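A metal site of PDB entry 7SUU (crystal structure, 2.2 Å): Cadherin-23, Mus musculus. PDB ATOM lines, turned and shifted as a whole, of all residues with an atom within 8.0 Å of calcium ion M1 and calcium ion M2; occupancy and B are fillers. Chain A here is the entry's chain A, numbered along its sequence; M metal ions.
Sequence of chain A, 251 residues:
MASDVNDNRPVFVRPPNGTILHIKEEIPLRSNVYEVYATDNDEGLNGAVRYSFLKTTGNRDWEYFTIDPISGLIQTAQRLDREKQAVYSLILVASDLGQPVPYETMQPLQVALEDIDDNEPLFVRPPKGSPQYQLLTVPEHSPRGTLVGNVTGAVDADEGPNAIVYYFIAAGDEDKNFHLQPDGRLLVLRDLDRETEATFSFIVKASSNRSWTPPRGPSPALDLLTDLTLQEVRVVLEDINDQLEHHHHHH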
ATOM      1  N   GLU A 140       0.910  22.850   5.211  1.00  0.00           N
ATOM      2  CA  GLU A 140       0.972  22.185   6.547  1.00  0.00           C
ATOM      3  C   GLU A 140      -0.044  22.856   7.480  1.00  0.00           C
ATOM      4  O   GLU A 140      -0.275  24.055   7.314  1.00  0.00           O
ATOM      5  CB  GLU A 140       2.384  22.292   7.144  1.00  0.00           C
ATOM      6  CG  GLU A 140       2.921  23.718   7.264  1.00  0.00           C
ATOM      7  CD  GLU A 140       4.206  23.833   8.098  1.00  0.00           C
ATOM      8  OE1 GLU A 140       4.534  22.874   8.812  1.00  0.00           O
ATOM      9  OE2 GLU A 140       4.890  24.858   7.989  1.00  0.00           O
ATOM     10  N   HIS A 141      -0.572  22.127   8.458  1.00  0.00           N
ATOM     11  CA  HIS A 141      -1.489  22.694   9.490  1.00  0.00           C
ATOM     12  C   HIS A 141      -2.837  23.107   8.882  1.00  0.00           C
ATOM     13  O   HIS A 141      -3.586  23.804   9.554  1.00  0.00           O
ATOM     14  CB  HIS A 141      -0.771  23.821  10.262  1.00  0.00           C
ATOM     15  CG  HIS A 141       0.514  23.390  10.919  1.00  0.00           C
ATOM     16  ND1 HIS A 141       0.572  22.351  11.840  1.00  0.00           N
ATOM     17  CD2 HIS A 141       1.779  23.834  10.792  1.00  0.00           C
ATOM     18  CE1 HIS A 141       1.813  22.174  12.250  1.00  0.00           C
ATOM     19  NE2 HIS A 141       2.574  23.087  11.646  1.00  0.00           N
ATOM     20  N   ASP A 191      -3.461  16.693  11.738  1.00  0.00           N
ATOM     21  CA  ASP A 191      -2.591  17.897  11.797  1.00  0.00           C
ATOM     22  C   ASP A 191      -1.257  17.536  11.143  1.00  0.00           C
ATOM     23  O   ASP A 191      -0.575  16.646  11.661  1.00  0.00           O
ATOM     24  CB  ASP A 191      -2.391  18.368  13.234  1.00  0.00           C
ATOM     25  CG  ASP A 191      -1.449  19.567  13.294  1.00  0.00           C
ATOM     26  OD1 ASP A 191      -1.512  20.420  12.366  1.00  0.00           O
ATOM     27  OD2 ASP A 191      -0.654  19.635  14.265  1.00  0.00           O
ATOM     28  N   LEU A 192      -0.913  18.175  10.035  1.00  0.00           N
ATOM     29  CA  LEU A 192       0.329  17.829   9.306  1.00  0.00           C
ATOM     30  C   LEU A 192       1.330  18.968   9.479  1.00  0.00           C
ATOM     31  O   LEU A 192       0.950  20.165   9.308  1.00  0.00           O
ATOM     32  CB  LEU A 192      -0.001  17.530   7.841  1.00  0.00           C
ATOM     33  CG  LEU A 192      -1.074  16.457   7.629  1.00  0.00           C
ATOM     34  CD1 LEU A 192      -1.235  16.174   6.153  1.00  0.00           C
ATOM     35  CD2 LEU A 192      -0.768  15.181   8.401  1.00  0.00           C
ATOM     36  N   ASP A 193       2.551  18.598   9.867  1.00  0.00           N
ATOM     37  CA  ASP A 193       3.636  19.518  10.289  1.00  0.00           C
ATOM     38  C   ASP A 193       4.844  19.309   9.375  1.00  0.00           C
ATOM     39  O   ASP A 193       5.347  18.170   9.319  1.00  0.00           O
ATOM     40  CB  ASP A 193       3.970  19.300  11.768  1.00  0.00           C
ATOM     41  CG  ASP A 193       5.193  20.103  12.169  1.00  0.00           C
ATOM     42  OD1 ASP A 193       5.361  21.241  11.635  1.00  0.00           O
ATOM     43  OD2 ASP A 193       5.992  19.570  12.973  1.00  0.00           O
ATOM     44  N   ARG A 194       5.250  20.357   8.657  1.00  0.00           N
ATOM     45  CA  ARG A 194       6.341  20.288   7.637  1.00  0.00           C
ATOM     46  C   ARG A 194       7.650  19.981   8.352  1.00  0.00           C
ATOM     47  O   ARG A 194       8.478  19.245   7.810  1.00  0.00           O
ATOM     48  CB  ARG A 194       6.487  21.620   6.889  1.00  0.00           C
ATOM     49  CG  ARG A 194       7.543  21.622   5.775  1.00  0.00           C
ATOM     50  CD  ARG A 194       7.608  22.989   5.134  1.00  0.00           C
ATOM     51  NE  ARG A 194       8.809  23.245   4.361  1.00  0.00           N
ATOM     52  CZ  ARG A 194       8.900  23.249   3.025  1.00  0.00           C
ATOM     53  NH1 ARG A 194       7.872  22.949   2.248  1.00  0.00           N
ATOM     54  NH2 ARG A 194      10.075  23.537   2.461  1.00  0.00           N
ATOM     55  N   GLU A 195       7.825  20.507   9.558  1.00  0.00           N
ATOM     56  CA  GLU A 195       9.084  20.418  10.328  1.00  0.00           C
ATOM     57  C   GLU A 195       9.206  19.047  11.020  1.00  0.00           C
ATOM     58  O   GLU A 195      10.206  18.890  11.723  1.00  0.00           O
ATOM     59  CB  GLU A 195       9.161  21.591  11.313  1.00  0.00           C
ATOM     60  CG  GLU A 195       9.464  22.923  10.633  1.00  0.00           C
ATOM     61  CD  GLU A 195       8.349  23.557   9.807  1.00  0.00           C
ATOM     62  OE1 GLU A 195       8.644  24.000   8.662  1.00  0.00           O
ATOM     63  OE2 GLU A 195       7.197  23.665  10.328  1.00  0.00           O
ATOM     64  N   THR A 196       8.300  18.094  10.776  1.00  0.00           N
ATOM     65  CA  THR A 196       8.332  16.739  11.384  1.00  0.00           C
ATOM     66  C   THR A 196       8.255  15.657  10.303  1.00  0.00           C
ATOM     67  O   THR A 196       9.105  14.750  10.319  1.00  0.00           O
ATOM     68  CB  THR A 196       7.193  16.529  12.393  1.00  0.00           C
ATOM     69  OG1 THR A 196       7.289  17.511  13.426  1.00  0.00           O
ATOM     70  CG2 THR A 196       7.217  15.164  13.049  1.00  0.00           C
ATOM     71  N   LEU A 237       4.121  18.884   1.936  1.00  0.00           N
ATOM     72  CA  LEU A 237       3.547  20.015   2.701  1.00  0.00           C
ATOM     73  C   LEU A 237       4.253  21.293   2.273  1.00  0.00           C
ATOM     74  O   LEU A 237       5.451  21.322   2.344  1.00  0.00           O
ATOM     75  CB  LEU A 237       3.701  19.785   4.220  1.00  0.00           C
ATOM     76  CG  LEU A 237       3.160  18.432   4.702  1.00  0.00           C
ATOM     77  CD1 LEU A 237       3.171  18.294   6.226  1.00  0.00           C
ATOM     78  CD2 LEU A 237       1.763  18.201   4.167  1.00  0.00           C
ATOM     79  N   GLU A 238       3.484  22.299   1.846  1.00  0.00           N
ATOM     80  CA  GLU A 238       3.973  23.670   1.565  1.00  0.00           C
ATOM     81  C   GLU A 238       4.280  24.336   2.913  1.00  0.00           C
ATOM     82  O   GLU A 238       3.505  24.136   3.891  1.00  0.00           O
ATOM     83  CB  GLU A 238       2.943  24.506   0.804  1.00  0.00           C
ATOM     84  CG  GLU A 238       2.553  23.933  -0.550  1.00  0.00           C
ATOM     85  CD  GLU A 238       1.348  24.643  -1.148  1.00  0.00           C
ATOM     86  OE1 GLU A 238       1.294  25.889  -1.028  1.00  0.00           O
ATOM     87  OE2 GLU A 238       0.452  23.958  -1.699  1.00  0.00           O
ATOM     88  N   ASP A 239       5.328  25.139   2.924  1.00  0.00           N
ATOM     89  CA  ASP A 239       5.822  25.855   4.127  1.00  0.00           C
ATOM     90  C   ASP A 239       4.818  26.933   4.521  1.00  0.00           C
ATOM     91  O   ASP A 239       4.379  27.674   3.653  1.00  0.00           O
ATOM     92  CB  ASP A 239       7.207  26.476   3.941  1.00  0.00           C
ATOM     93  CG  ASP A 239       7.803  26.914   5.272  1.00  0.00           C
ATOM     94  OD1 ASP A 239       7.748  26.142   6.217  1.00  0.00           O
ATOM     95  OD2 ASP A 239       8.222  28.069   5.371  1.00  0.00           O
ATOM     96  N   ILE A 240       4.456  26.945   5.795  1.00  0.00           N
ATOM     97  CA  ILE A 240       3.841  28.078   6.534  1.00  0.00           C
ATOM     98  C   ILE A 240       4.931  28.652   7.446  1.00  0.00           C
ATOM     99  O   ILE A 240       5.795  27.864   7.952  1.00  0.00           O
ATOM    100  CB  ILE A 240       2.579  27.596   7.283  1.00  0.00           C
ATOM    101  CG1 ILE A 240       1.312  28.033   6.548  1.00  0.00           C
ATOM    102  CG2 ILE A 240       2.520  28.024   8.730  1.00  0.00           C
ATOM    103  CD1 ILE A 240       1.124  27.313   5.251  1.00  0.00           C
ATOM    104  N   ASN A 241       4.888  29.964   7.654  1.00  0.00           N
ATOM    105  CA  ASN A 241       5.801  30.652   8.611  1.00  0.00           C
ATOM    106  C   ASN A 241       5.235  30.511  10.038  1.00  0.00           C
ATOM    107  O   ASN A 241       4.516  31.421  10.478  1.00  0.00           O
ATOM    108  CB  ASN A 241       6.038  32.085   8.146  1.00  0.00           C
ATOM    109  CG  ASN A 241       7.204  32.734   8.848  1.00  0.00           C
ATOM    110  OD1 ASN A 241       7.849  32.131   9.715  1.00  0.00           O
ATOM    111  ND2 ASN A 241       7.471  33.988   8.497  1.00  0.00           N
ATOM    112  N   ASP A 242       5.563  29.403  10.743  1.00  0.00           N
ATOM    113  CA  ASP A 242       4.975  28.986  12.061  1.00  0.00           C
ATOM    114  C   ASP A 242       6.067  28.968  13.137  1.00  0.00           C
ATOM    115  O   ASP A 242       7.218  29.411  12.961  1.00  0.00           O
ATOM    116  CB  ASP A 242       4.235  27.638  11.974  1.00  0.00           C
ATOM    117  CG  ASP A 242       4.940  26.470  11.275  1.00  0.00           C
ATOM    118  OD1 ASP A 242       5.904  26.684  10.517  1.00  0.00           O
ATOM    119  OD2 ASP A 242       4.511  25.323  11.496  1.00  0.00           O
HETATM  120 CA    CA M   1       7.041  26.032   8.493  1.00  0.00          CA
HETATM  121 CA    CA M   2       5.170  23.447  11.280  1.00  0.00          CA
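The side-chain carboxylate (OD2) of Asp 193 lies within hydrogen-bond range of the side-chain hydroxyl (OG1) of Thr 196, at 2.5 Å. The side-chain carboxylate (OD1) of Asp 239 sits close to the guanidinium group (NE) of Arg 194 (3.6 Å). OE1 of Glu 140 lies close to N of Arg 194. N of Glu 140 lies within hydrogen-bond range of O of Glu 238 (3.2 Å). The backbone NH of His 141 is in hydrogen-bond range of the backbone carbonyl oxygen of Leu 192 (2.6 Å). The side-chain carboxylate (OD1) of Asp 191 lies within hydrogen-bond range of a ring nitrogen (ND1) of His 141 (2.9 Å).
Within 4 Å of calcium ion M1: Glu 140, Glu 195, Asp 239, Ile 240 and Asp 242.
Five residues have an atom within 4 Å of calcium ion M2: Glu 140, His 141, Asp 193, Glu 195 and Asp 242. Along chain A the residues within 4 Å of calcium ion M2 span positions 140 to 242.
Calcium ion M2 is bound by OD2 of Asp 242, OD1 of Asp 193, OE2 of Glu 195, OE1 of Glu 140 and NE2 of His 141. Calcium ion M2 has five donor atoms within binding distance.
Calcium ion M1 is bound by the backbone carbonyl oxygen of Ile 240 (2.3 Å), the side-chain carboxylate of Asp 239 (2.4 Å), the side-chain carboxylate of Asp 242 (2.4 Å), the side-chain carboxylate of Glu 140 (2.5 Å) and the side-chain carboxylate of Glu 195 (2.6 Å). Slightly farther from calcium ion M1 lies the side-chain carboxylate (OE2) of Glu 195 (3.0 Å).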
